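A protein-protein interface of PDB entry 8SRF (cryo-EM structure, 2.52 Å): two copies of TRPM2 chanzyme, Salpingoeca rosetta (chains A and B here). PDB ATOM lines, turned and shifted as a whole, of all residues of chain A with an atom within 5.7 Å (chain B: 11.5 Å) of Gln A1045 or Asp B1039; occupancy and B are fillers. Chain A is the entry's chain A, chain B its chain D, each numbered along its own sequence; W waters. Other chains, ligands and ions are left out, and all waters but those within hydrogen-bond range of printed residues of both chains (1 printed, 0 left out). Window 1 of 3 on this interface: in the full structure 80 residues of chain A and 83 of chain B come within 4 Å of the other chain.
NE2 of Gln A1045 sits at hydrogen-bond distance from OD2 of Asp B1039 (2.9 Å). The side-chain amide oxygen (OD1) of Asn A1038 lies within hydrogen-bond range of the side-chain amide nitrogen (ND2) of Asn B1038, at 3.3 Å.
The backbone carbonyl oxygen (O) of Ile B1034 lies within hydrogen-bond range of the side-chain amide nitrogen (ND2) of Asn B1038, at 2.8 Å. O of Met B1036 sits at hydrogen-bond distance from OG1 of Thr B1040, at 2.4 Å. The side-chain amino group (NZ) of Lys B1043 lies within salt-bridge range of the side-chain carboxylate (OD1) of Asp B1039, 3.5 Å away.
Asn A1038 touches its own counterpart, Asn B1038. Positions printed for both chains: 930, 1038, 1040, 1041, 1042, 1043, 1044, 1045, 1046, 1047 and 1048.
Of the printed residues of chain B, Asn A1038 touches Ala B1035 (3.4 Å) and Asn B1038 (3.3 Å). Of the printed residues of chain B, Tyr A1041 touches Ala B1035, Met B1036 and Asp B1039. No residue of chain B comes within 4 Å of Val A1044. Of chain B, only Asp B1039 comes within 4 Å of Gln A1045. No residue of chain B comes within 4 Å of Glu A1046. No residue of chain B comes within 4 Å of Ala A1047. Ala A1048 touches none of the printed residues of chain B. No residue of chain B comes within 4 Å of Glu A1049. Glu B933 touches none of the printed residues of chain A. Of the printed residues of chain A, Ala B1035 touches Asn A1038 and Tyr A1041. Printed residues of chain A within 4 Å of Asn B1038: Asn A1038 (3.3 Å). Printed residues of chain A within 4 Å of Asp B1039: Tyr A1041 and Gln A1045. The nearest residue of chain B that does not touch Gln A1045 is Lys B1043 (4.02 Å). The nearest residue of chain A that does not touch Asp B1039 is Met A1042 (5.1 Å). The nearest printed residue of chain B that does not touch Tyr A1041 is Leu B1032 (4.2 Å).
Printed residues of chain B that touch a printed residue of chain A: Ala B1035, Met B1036, Asn B1038 and Asp B1039. Among the printed residues, 6 pairs touch across the chains. Among the printed residues, no Asp or Glu carboxylate lies within 4 Å of a Lys or Arg side-chain nitrogen of the other chain.
Water W1 lies within hydrogen-bond range of the backbone carbonyl oxygen of Ala B1035 and the side-chain amide oxygen of Asn A1038.
Among the printed residues, merely in contact across the chains: Tyr A1041 with Met B1036 (3.4 Å), Asn A1038 with Ala B1035 (3.4 Å), Tyr A1041 with Asp B1039 (3.5 Å) and Tyr A1041 with Ala B1035 (3.997 Å).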
ATOM      1  N   MET A 930     -11.802  -5.583 -29.681  1.00  0.00           N
ATOM      2  CA  MET A 930     -11.341  -4.627 -30.719  1.00  0.00           C
ATOM      3  C   MET A 930      -9.836  -4.756 -30.952  1.00  0.00           C
ATOM      4  O   MET A 930      -9.433  -4.688 -32.104  1.00  0.00           O
ATOM      5  CB  MET A 930     -11.660  -3.184 -30.338  1.00  0.00           C
ATOM      6  CG  MET A 930     -11.733  -2.259 -31.525  1.00  0.00           C
ATOM      7  SD  MET A 930     -13.442  -1.995 -32.022  1.00  0.00           S
ATOM      8  CE  MET A 930     -14.231  -1.937 -30.416  1.00  0.00           C
ATOM      9  N   ASN A1038      -9.139   4.099 -37.020  1.00  0.00           N
ATOM     10  CA  ASN A1038     -10.383   4.865 -36.841  1.00  0.00           C
ATOM     11  C   ASN A1038     -11.545   4.301 -37.648  1.00  0.00           C
ATOM     12  O   ASN A1038     -12.658   4.144 -37.107  1.00  0.00           O
ATOM     13  CB  ASN A1038     -10.167   6.313 -37.250  1.00  0.00           C
ATOM     14  CG  ASN A1038      -9.629   7.155 -36.145  1.00  0.00           C
ATOM     15  OD1 ASN A1038     -10.299   7.427 -35.155  1.00  0.00           O
ATOM     16  ND2 ASN A1038      -8.385   7.538 -36.282  1.00  0.00           N
ATOM     17  N   THR A1040     -11.681   1.131 -38.935  1.00  0.00           N
ATOM     18  CA  THR A1040     -11.874  -0.229 -38.439  1.00  0.00           C
ATOM     19  C   THR A1040     -12.712  -0.242 -37.167  1.00  0.00           C
ATOM     20  O   THR A1040     -13.654  -1.041 -37.090  1.00  0.00           O
ATOM     21  CB  THR A1040     -10.501  -0.865 -38.211  1.00  0.00           C
ATOM     22  OG1 THR A1040      -9.808  -0.942 -39.461  1.00  0.00           O
ATOM     23  CG2 THR A1040     -10.578  -2.284 -37.645  1.00  0.00           C
ATOM     24  N   TYR A1041     -12.430   0.719 -36.243  1.00  0.00           N
ATOM     25  CA  TYR A1041     -13.131   0.931 -34.962  1.00  0.00           C
ATOM     26  C   TYR A1041     -14.615   1.229 -35.188  1.00  0.00           C
ATOM     27  O   TYR A1041     -15.479   0.602 -34.539  1.00  0.00           O
ATOM     28  CB  TYR A1041     -12.441   2.059 -34.176  1.00  0.00           C
ATOM     29  CG  TYR A1041     -12.821   2.150 -32.702  1.00  0.00           C
ATOM     30  CD1 TYR A1041     -13.916   2.934 -32.263  1.00  0.00           C
ATOM     31  CD2 TYR A1041     -12.065   1.451 -31.739  1.00  0.00           C
ATOM     32  CE1 TYR A1041     -14.261   2.985 -30.924  1.00  0.00           C
ATOM     33  CE2 TYR A1041     -12.408   1.509 -30.376  1.00  0.00           C
ATOM     34  CZ  TYR A1041     -13.503   2.298 -30.002  1.00  0.00           C
ATOM     35  OH  TYR A1041     -13.904   2.407 -28.705  1.00  0.00           O
ATOM     36  N   MET A1042     -14.901   2.224 -36.074  1.00  0.00           N
ATOM     37  CA  MET A1042     -16.275   2.594 -36.458  1.00  0.00           C
ATOM     38  C   MET A1042     -17.016   1.436 -37.145  1.00  0.00           C
ATOM     39  O   MET A1042     -18.242   1.327 -37.026  1.00  0.00           O
ATOM     40  CB  MET A1042     -16.297   3.836 -37.350  1.00  0.00           C
ATOM     41  CG  MET A1042     -15.855   5.119 -36.668  1.00  0.00           C
ATOM     42  SD  MET A1042     -15.971   6.569 -37.740  1.00  0.00           S
ATOM     43  CE  MET A1042     -14.592   6.332 -38.854  1.00  0.00           C
ATOM     44  N   LYS A1043     -16.288   0.589 -37.895  1.00  0.00           N
ATOM     45  CA  LYS A1043     -16.919  -0.524 -38.600  1.00  0.00           C
ATOM     46  C   LYS A1043     -17.301  -1.661 -37.648  1.00  0.00           C
ATOM     47  O   LYS A1043     -18.385  -2.239 -37.787  1.00  0.00           O
ATOM     48  CB  LYS A1043     -16.025  -1.047 -39.723  1.00  0.00           C
ATOM     49  CG  LYS A1043     -16.110  -0.252 -41.017  1.00  0.00           C
ATOM     50  CD  LYS A1043     -15.106  -0.761 -42.041  1.00  0.00           C
ATOM     51  CE  LYS A1043     -15.342  -0.183 -43.435  1.00  0.00           C
ATOM     52  NZ  LYS A1043     -16.208   1.033 -43.453  1.00  0.00           N
ATOM     53  N   VAL A1044     -16.449  -2.006 -36.670  1.00  0.00           N
ATOM     54  CA  VAL A1044     -16.623  -3.286 -35.966  1.00  0.00           C
ATOM     55  C   VAL A1044     -16.939  -3.116 -34.471  1.00  0.00           C
ATOM     56  O   VAL A1044     -16.907  -4.122 -33.737  1.00  0.00           O
ATOM     57  CB  VAL A1044     -15.440  -4.279 -36.182  1.00  0.00           C
ATOM     58  CG1 VAL A1044     -15.226  -4.617 -37.665  1.00  0.00           C
ATOM     59  CG2 VAL A1044     -14.078  -3.931 -35.481  1.00  0.00           C
ATOM     60  N   GLN A1045     -17.291  -1.882 -34.016  1.00  0.00           N
ATOM     61  CA  GLN A1045     -17.684  -1.619 -32.615  1.00  0.00           C
ATOM     62  C   GLN A1045     -18.956  -2.368 -32.163  1.00  0.00           C
ATOM     63  O   GLN A1045     -18.971  -2.955 -31.067  1.00  0.00           O
ATOM     64  CB  GLN A1045     -17.872  -0.112 -32.434  1.00  0.00           C
ATOM     65  CG  GLN A1045     -17.539   0.412 -31.058  1.00  0.00           C
ATOM     66  CD  GLN A1045     -17.739   1.908 -30.952  1.00  0.00           C
ATOM     67  OE1 GLN A1045     -17.809   2.609 -31.962  1.00  0.00           O
ATOM     68  NE2 GLN A1045     -17.833   2.406 -29.726  1.00  0.00           N
ATOM     69  N   GLU A1046     -19.998  -2.398 -33.017  1.00  0.00           N
ATOM     70  CA  GLU A1046     -21.257  -3.093 -32.711  1.00  0.00           C
ATOM     71  C   GLU A1046     -21.077  -4.614 -32.725  1.00  0.00           C
ATOM     72  O   GLU A1046     -21.678  -5.333 -31.907  1.00  0.00           O
ATOM     73  CB  GLU A1046     -22.341  -2.676 -33.702  1.00  0.00           C
ATOM     74  CG  GLU A1046     -22.370  -1.181 -33.989  1.00  0.00           C
ATOM     75  CD  GLU A1046     -22.972  -0.370 -32.853  1.00  0.00           C
ATOM     76  OE1 GLU A1046     -23.888  -0.877 -32.173  1.00  0.00           O
ATOM     77  OE2 GLU A1046     -22.527   0.779 -32.640  1.00  0.00           O
ATOM     78  N   ALA A1047     -20.265  -5.097 -33.681  1.00  0.00           N
ATOM     79  CA  ALA A1047     -19.872  -6.502 -33.785  1.00  0.00           C
ATOM     80  C   ALA A1047     -19.049  -6.955 -32.584  1.00  0.00           C
ATOM     81  O   ALA A1047     -19.145  -8.118 -32.174  1.00  0.00           O
ATOM     82  CB  ALA A1047     -19.095  -6.726 -35.081  1.00  0.00           C
ATOM     83  N   ALA A1048     -18.179  -6.066 -32.071  1.00  0.00           N
ATOM     84  CA  ALA A1048     -17.411  -6.321 -30.851  1.00  0.00           C
ATOM     85  C   ALA A1048     -18.309  -6.449 -29.626  1.00  0.00           C
ATOM     86  O   ALA A1048     -18.015  -7.262 -28.738  1.00  0.00           O
ATOM     87  CB  ALA A1048     -16.379  -5.220 -30.644  1.00  0.00           C
ATOM     88  N   GLU A1049     -19.355  -5.597 -29.536  1.00  0.00           N
ATOM     89  CA  GLU A1049     -20.358  -5.688 -28.460  1.00  0.00           C
ATOM     90  C   GLU A1049     -21.140  -7.006 -28.519  1.00  0.00           C
ATOM     91  O   GLU A1049     -21.410  -7.623 -27.474  1.00  0.00           O
ATOM     92  CB  GLU A1049     -21.311  -4.493 -28.483  1.00  0.00           C
ATOM     93  CG  GLU A1049     -20.654  -3.165 -28.161  1.00  0.00           C
ATOM     94  CD  GLU A1049     -20.617  -2.882 -26.674  1.00  0.00           C
ATOM     95  OE1 GLU A1049     -21.396  -3.511 -25.931  1.00  0.00           O
ATOM     96  OE2 GLU A1049     -19.805  -2.033 -26.248  1.00  0.00           O
ATOM     97  N   ASP A1050     -21.539  -7.413 -29.745  1.00  0.00           N
ATOM     98  CA  ASP A1050     -22.238  -8.679 -30.002  1.00  0.00           C
ATOM     99  C   ASP A1050     -21.362  -9.888 -29.658  1.00  0.00           C
ATOM    100  O   ASP A1050     -21.849 -10.878 -29.083  1.00  0.00           O
ATOM    101  CB  ASP A1050     -22.672  -8.737 -31.465  1.00  0.00           C
ATOM    102  CG  ASP A1050     -23.846  -7.825 -31.763  1.00  0.00           C
ATOM    103  OD1 ASP A1050     -24.534  -7.401 -30.812  1.00  0.00           O
ATOM    104  OD2 ASP A1050     -24.078  -7.527 -32.952  1.00  0.00           O
ATOM    105  N   MET B 930     -15.321  17.503 -21.684  1.00  0.00           N
ATOM    106  CA  MET B 930     -14.861  16.374 -22.532  1.00  0.00           C
ATOM    107  C   MET B 930     -13.634  15.697 -21.924  1.00  0.00           C
ATOM    108  O   MET B 930     -13.577  14.476 -21.976  1.00  0.00           O
ATOM    109  CB  MET B 930     -14.521  16.836 -23.946  1.00  0.00           C
ATOM    110  CG  MET B 930     -14.590  15.727 -24.965  1.00  0.00           C
ATOM    111  SD  MET B 930     -16.156  15.772 -25.849  1.00  0.00           S
ATOM    112  CE  MET B 930     -16.384  17.542 -25.997  1.00  0.00           C
ATOM    113  N   GLU B 933     -14.603  13.264 -19.388  1.00  0.00           N
ATOM    114  CA  GLU B 933     -15.186  12.095 -20.054  1.00  0.00           C
ATOM    115  C   GLU B 933     -14.096  11.190 -20.649  1.00  0.00           C
ATOM    116  O   GLU B 933     -14.198   9.961 -20.559  1.00  0.00           O
ATOM    117  CB  GLU B 933     -16.212  12.498 -21.105  1.00  0.00           C
ATOM    118  CG  GLU B 933     -17.308  11.447 -21.230  1.00  0.00           C
ATOM    119  CD  GLU B 933     -18.341  11.505 -20.112  1.00  0.00           C
ATOM    120  OE1 GLU B 933     -18.508  12.572 -19.483  1.00  0.00           O
ATOM    121  OE2 GLU B 933     -18.992  10.469 -19.858  1.00  0.00           O
ATOM    122  N   MET B 934     -13.057  11.776 -21.291  1.00  0.00           N
ATOM    123  CA  MET B 934     -11.923  11.020 -21.873  1.00  0.00           C
ATOM    124  C   MET B 934     -11.020  10.337 -20.837  1.00  0.00           C
ATOM    125  O   MET B 934     -10.195   9.503 -21.246  1.00  0.00           O
ATOM    126  CB  MET B 934     -11.006  11.837 -22.795  1.00  0.00           C
ATOM    127  CG  MET B 934     -11.621  12.603 -23.921  1.00  0.00           C
ATOM    128  SD  MET B 934     -12.293  11.822 -25.373  1.00  0.00           S
ATOM    129  CE  MET B 934     -11.836  13.090 -26.538  1.00  0.00           C
ATOM    130  N   ASP B 937     -11.417   6.545 -20.889  1.00  0.00           N
ATOM    131  CA  ASP B 937     -10.614   5.980 -21.980  1.00  0.00           C
ATOM    132  C   ASP B 937      -9.136   5.903 -21.624  1.00  0.00           C
ATOM    133  O   ASP B 937      -8.444   4.961 -22.047  1.00  0.00           O
ATOM    134  CB  ASP B 937     -10.784   6.818 -23.239  1.00  0.00           C
ATOM    135  CG  ASP B 937     -12.144   6.677 -23.846  1.00  0.00           C
ATOM    136  OD1 ASP B 937     -12.847   5.690 -23.550  1.00  0.00           O
ATOM    137  OD2 ASP B 937     -12.505   7.565 -24.627  1.00  0.00           O
ATOM    138  N   THR B 940      -8.849   2.994 -19.225  1.00  0.00           N
ATOM    139  CA  THR B 940      -8.925   1.779 -20.049  1.00  0.00           C
ATOM    140  C   THR B 940      -7.571   1.464 -20.697  1.00  0.00           C
ATOM    141  O   THR B 940      -7.134   0.297 -20.695  1.00  0.00           O
ATOM    142  CB  THR B 940     -10.028   1.974 -21.104  1.00  0.00           C
ATOM    143  OG1 THR B 940     -11.284   2.161 -20.441  1.00  0.00           O
ATOM    144  CG2 THR B 940     -10.176   0.784 -22.052  1.00  0.00           C
ATOM    145  N   VAL B1030      -1.630   2.988 -28.403  1.00  0.00           N
ATOM    146  CA  VAL B1030      -1.711   4.450 -28.550  1.00  0.00           C
ATOM    147  C   VAL B1030      -2.655   4.839 -29.694  1.00  0.00           C
ATOM    148  O   VAL B1030      -3.495   5.738 -29.539  1.00  0.00           O
ATOM    149  CB  VAL B1030      -0.281   5.026 -28.700  1.00  0.00           C
ATOM    150  CG1 VAL B1030      -0.224   6.438 -29.285  1.00  0.00           C
ATOM    151  CG2 VAL B1030       0.397   5.065 -27.346  1.00  0.00           C
ATOM    152  N   ASN B1031      -2.562   4.128 -30.828  1.00  0.00           N
ATOM    153  CA  ASN B1031      -3.411   4.364 -31.999  1.00  0.00           C
ATOM    154  C   ASN B1031      -4.867   3.953 -31.733  1.00  0.00           C
ATOM    155  O   ASN B1031      -5.807   4.596 -32.239  1.00  0.00           O
ATOM    156  CB  ASN B1031      -2.818   3.622 -33.191  1.00  0.00           C
ATOM    157  CG  ASN B1031      -1.494   4.202 -33.627  1.00  0.00           C
ATOM    158  OD1 ASN B1031      -1.277   5.405 -33.556  1.00  0.00           O
ATOM    159  ND2 ASN B1031      -0.599   3.340 -34.088  1.00  0.00           N
ATOM    160  N   LEU B1032      -5.044   2.867 -30.950  1.00  0.00           N
ATOM    161  CA  LEU B1032      -6.352   2.428 -30.447  1.00  0.00           C
ATOM    162  C   LEU B1032      -6.981   3.473 -29.540  1.00  0.00           C
ATOM    163  O   LEU B1032      -8.191   3.704 -29.627  1.00  0.00           O
ATOM    164  CB  LEU B1032      -6.231   1.105 -29.685  1.00  0.00           C
ATOM    165  CG  LEU B1032      -7.350   0.513 -28.815  1.00  0.00           C
ATOM    166  CD1 LEU B1032      -8.559   0.111 -29.631  1.00  0.00           C
ATOM    167  CD2 LEU B1032      -6.833  -0.666 -28.010  1.00  0.00           C
ATOM    168  N   LEU B1033      -6.151   4.113 -28.688  1.00  0.00           N
ATOM    169  CA  LEU B1033      -6.566   5.207 -27.802  1.00  0.00           C
ATOM    170  C   LEU B1033      -7.028   6.433 -28.597  1.00  0.00           C
ATOM    171  O   LEU B1033      -7.980   7.107 -28.176  1.00  0.00           O
ATOM    172  CB  LEU B1033      -5.442   5.558 -26.828  1.00  0.00           C
ATOM    173  CG  LEU B1033      -5.711   6.583 -25.735  1.00  0.00           C
ATOM    174  CD1 LEU B1033      -6.911   6.120 -24.923  1.00  0.00           C
ATOM    175  CD2 LEU B1033      -4.509   6.811 -24.907  1.00  0.00           C
ATOM    176  N   ILE B1034      -6.338   6.728 -29.726  1.00  0.00           N
ATOM    177  CA  ILE B1034      -6.703   7.810 -30.666  1.00  0.00           C
ATOM    178  C   ILE B1034      -8.088   7.539 -31.269  1.00  0.00           C
ATOM    179  O   ILE B1034      -8.937   8.451 -31.332  1.00  0.00           O
ATOM    180  CB  ILE B1034      -5.606   7.991 -31.747  1.00  0.00           C
ATOM    181  CG1 ILE B1034      -4.326   8.553 -31.139  1.00  0.00           C
ATOM    182  CG2 ILE B1034      -6.011   8.903 -32.911  1.00  0.00           C
ATOM    183  CD1 ILE B1034      -3.114   8.522 -32.051  1.00  0.00           C
ATOM    184  N   ALA B1035      -8.333   6.267 -31.664  1.00  0.00           N
ATOM    185  CA  ALA B1035      -9.632   5.818 -32.196  1.00  0.00           C
ATOM    186  C   ALA B1035     -10.772   5.918 -31.163  1.00  0.00           C
ATOM    187  O   ALA B1035     -11.885   6.357 -31.510  1.00  0.00           O
ATOM    188  CB  ALA B1035      -9.509   4.387 -32.713  1.00  0.00           C
ATOM    189  N   MET B1036     -10.493   5.513 -29.900  1.00  0.00           N
ATOM    190  CA  MET B1036     -11.445   5.626 -28.782  1.00  0.00           C
ATOM    191  C   MET B1036     -11.771   7.079 -28.446  1.00  0.00           C
ATOM    192  O   MET B1036     -12.926   7.391 -28.124  1.00  0.00           O
ATOM    193  CB  MET B1036     -10.922   4.914 -27.530  1.00  0.00           C
ATOM    194  CG  MET B1036     -10.838   3.407 -27.628  1.00  0.00           C
ATOM    195  SD  MET B1036      -9.769   2.623 -26.406  1.00  0.00           S
ATOM    196  CE  MET B1036     -10.234   3.466 -24.914  1.00  0.00           C
ATOM    197  N   PHE B1037     -10.749   7.956 -28.483  1.00  0.00           N
ATOM    198  CA  PHE B1037     -10.908   9.397 -28.263  1.00  0.00           C
ATOM    199  C   PHE B1037     -11.772  10.065 -29.329  1.00  0.00           C
ATOM    200  O   PHE B1037     -12.622  10.897 -28.987  1.00  0.00           O
ATOM    201  CB  PHE B1037      -9.534  10.061 -28.211  1.00  0.00           C
ATOM    202  CG  PHE B1037      -8.995  10.279 -26.823  1.00  0.00           C
ATOM    203  CD1 PHE B1037      -8.908   9.232 -25.889  1.00  0.00           C
ATOM    204  CD2 PHE B1037      -8.500  11.542 -26.480  1.00  0.00           C
ATOM    205  CE1 PHE B1037      -8.372   9.466 -24.602  1.00  0.00           C
ATOM    206  CE2 PHE B1037      -7.956  11.782 -25.214  1.00  0.00           C
ATOM    207  CZ  PHE B1037      -7.870  10.732 -24.290  1.00  0.00           C
ATOM    208  N   ASN B1038     -11.556   9.710 -30.617  1.00  0.00           N
ATOM    209  CA  ASN B1038     -12.339  10.258 -31.736  1.00  0.00           C
ATOM    210  C   ASN B1038     -13.803   9.841 -31.694  1.00  0.00           C
ATOM    211  O   ASN B1038     -14.696  10.694 -31.868  1.00  0.00           O
ATOM    212  CB  ASN B1038     -11.743   9.805 -33.059  1.00  0.00           C
ATOM    213  CG  ASN B1038     -10.651  10.695 -33.541  1.00  0.00           C
ATOM    214  OD1 ASN B1038     -10.870  11.842 -33.916  1.00  0.00           O
ATOM    215  ND2 ASN B1038      -9.446  10.188 -33.490  1.00  0.00           N
ATOM    216  N   ASP B1039     -14.035   8.548 -31.396  1.00  0.00           N
ATOM    217  CA  ASP B1039     -15.375   7.971 -31.259  1.00  0.00           C
ATOM    218  C   ASP B1039     -16.126   8.554 -30.072  1.00  0.00           C
ATOM    219  O   ASP B1039     -17.315   8.886 -30.192  1.00  0.00           O
ATOM    220  CB  ASP B1039     -15.281   6.468 -31.131  1.00  0.00           C
ATOM    221  CG  ASP B1039     -16.635   5.815 -30.999  1.00  0.00           C
ATOM    222  OD1 ASP B1039     -17.469   5.996 -31.910  1.00  0.00           O
ATOM    223  OD2 ASP B1039     -16.865   5.125 -29.986  1.00  0.00           O
ATOM    224  N   THR B1040     -15.423   8.653 -28.922  1.00  0.00           N
ATOM    225  CA  THR B1040     -15.942   9.183 -27.663  1.00  0.00           C
ATOM    226  C   THR B1040     -16.332  10.649 -27.798  1.00  0.00           C
ATOM    227  O   THR B1040     -17.435  11.008 -27.365  1.00  0.00           O
ATOM    228  CB  THR B1040     -14.884   8.984 -26.577  1.00  0.00           C
ATOM    229  OG1 THR B1040     -14.648   7.582 -26.405  1.00  0.00           O
ATOM    230  CG2 THR B1040     -15.300   9.545 -25.216  1.00  0.00           C
ATOM    231  N   TYR B1041     -15.477  11.445 -28.498  1.00  0.00           N
ATOM    232  CA  TYR B1041     -15.662  12.878 -28.796  1.00  0.00           C
ATOM    233  C   TYR B1041     -16.940  13.113 -29.605  1.00  0.00           C
ATOM    234  O   TYR B1041     -17.751  13.993 -29.243  1.00  0.00           O
ATOM    235  CB  TYR B1041     -14.422  13.419 -29.527  1.00  0.00           C
ATOM    236  CG  TYR B1041     -14.312  14.939 -29.581  1.00  0.00           C
ATOM    237  CD1 TYR B1041     -14.881  15.690 -30.638  1.00  0.00           C
ATOM    238  CD2 TYR B1041     -13.617  15.627 -28.566  1.00  0.00           C
ATOM    239  CE1 TYR B1041     -14.791  17.070 -30.657  1.00  0.00           C
ATOM    240  CE2 TYR B1041     -13.516  17.030 -28.587  1.00  0.00           C
ATOM    241  CZ  TYR B1041     -14.102  17.719 -29.656  1.00  0.00           C
ATOM    242  OH  TYR B1041     -14.054  19.076 -29.754  1.00  0.00           O
ATOM    243  N   MET B1042     -17.088  12.356 -30.728  1.00  0.00           N
ATOM    244  CA  MET B1042     -18.287  12.406 -31.584  1.00  0.00           C
ATOM    245  C   MET B1042     -19.555  11.975 -30.831  1.00  0.00           C
ATOM    246  O   MET B1042     -20.651  12.460 -31.134  1.00  0.00           O
ATOM    247  CB  MET B1042     -18.113  11.564 -32.849  1.00  0.00           C
ATOM    248  CG  MET B1042     -17.068  12.082 -33.821  1.00  0.00           C
ATOM    249  SD  MET B1042     -16.955  11.096 -35.332  1.00  0.00           S
ATOM    250  CE  MET B1042     -16.127   9.617 -34.762  1.00  0.00           C
ATOM    251  N   LYS B1043     -19.423  11.039 -29.874  1.00  0.00           N
ATOM    252  CA  LYS B1043     -20.582  10.557 -29.127  1.00  0.00           C
ATOM    253  C   LYS B1043     -21.059  11.580 -28.092  1.00  0.00           C
ATOM    254  O   LYS B1043     -22.271  11.775 -27.937  1.00  0.00           O
ATOM    255  CB  LYS B1043     -20.291   9.216 -28.457  1.00  0.00           C
ATOM    256  CG  LYS B1043     -20.448   8.010 -29.369  1.00  0.00           C
ATOM    257  CD  LYS B1043     -20.026   6.729 -28.664  1.00  0.00           C
ATOM    258  CE  LYS B1043     -20.424   5.472 -29.436  1.00  0.00           C
ATOM    259  NZ  LYS B1043     -20.764   5.719 -30.869  1.00  0.00           N
ATOM    260  N   VAL B1044     -20.149  12.253 -27.373  1.00  0.00           N
ATOM    261  CA  VAL B1044     -20.564  12.976 -26.160  1.00  0.00           C
ATOM    262  C   VAL B1044     -20.362  14.496 -26.263  1.00  0.00           C
ATOM    263  O   VAL B1044     -20.487  15.185 -25.232  1.00  0.00           O
ATOM    264  CB  VAL B1044     -19.928  12.411 -24.853  1.00  0.00           C
ATOM    265  CG1 VAL B1044     -20.278  10.932 -24.626  1.00  0.00           C
ATOM    266  CG2 VAL B1044     -18.394  12.666 -24.636  1.00  0.00           C
ATOM    267  N   GLN B1045     -20.105  15.037 -27.485  1.00  0.00           N
ATOM    268  CA  GLN B1045     -19.964  16.492 -27.712  1.00  0.00           C
ATOM    269  C   GLN B1045     -21.236  17.308 -27.397  1.00  0.00           C
ATOM    270  O   GLN B1045     -21.150  18.356 -26.734  1.00  0.00           O
ATOM    271  CB  GLN B1045     -19.540  16.723 -29.163  1.00  0.00           C
ATOM    272  CG  GLN B1045     -18.668  17.934 -29.388  1.00  0.00           C
ATOM    273  CD  GLN B1045     -18.280  18.097 -30.841  1.00  0.00           C
ATOM    274  OE1 GLN B1045     -18.376  17.156 -31.630  1.00  0.00           O
ATOM    275  NE2 GLN B1045     -17.839  19.295 -31.205  1.00  0.00           N
ATOM    276  N   GLU B1046     -22.416  16.810 -27.817  1.00  0.00           N
ATOM    277  CA  GLU B1046     -23.699  17.482 -27.564  1.00  0.00           C
ATOM    278  C   GLU B1046     -24.087  17.413 -26.085  1.00  0.00           C
ATOM    279  O   GLU B1046     -24.648  18.374 -25.530  1.00  0.00           O
ATOM    280  CB  GLU B1046     -24.794  16.867 -28.432  1.00  0.00           C
ATOM    281  CG  GLU B1046     -24.366  16.603 -29.869  1.00  0.00           C
ATOM    282  CD  GLU B1046     -24.289  17.868 -30.708  1.00  0.00           C
ATOM    283  OE1 GLU B1046     -25.094  18.794 -30.472  1.00  0.00           O
ATOM    284  OE2 GLU B1046     -23.421  17.938 -31.606  1.00  0.00           O
ATOM    285  N   ALA B1047     -23.807  16.255 -25.461  1.00  0.00           N
ATOM    286  CA  ALA B1047     -23.991  16.036 -24.027  1.00  0.00           C
ATOM    287  C   ALA B1047     -23.081  16.931 -23.192  1.00  0.00           C
ATOM    288  O   ALA B1047     -23.467  17.349 -22.094  1.00  0.00           O
ATOM    289  CB  ALA B1047     -23.746  14.565 -23.694  1.00  0.00           C
ATOM    290  N   ALA B1048     -21.843  17.157 -23.669  1.00  0.00           N
ATOM    291  CA  ALA B1048     -20.906  18.086 -23.036  1.00  0.00           C
ATOM    292  C   ALA B1048     -21.405  19.525 -23.088  1.00  0.00           C
ATOM    293  O   ALA B1048     -21.184  20.282 -22.132  1.00  0.00           O
ATOM    294  CB  ALA B1048     -19.536  17.972 -23.688  1.00  0.00           C
HETATM  295  O   HOH W   1     -12.597   6.122 -33.987  1.00  0.00           O
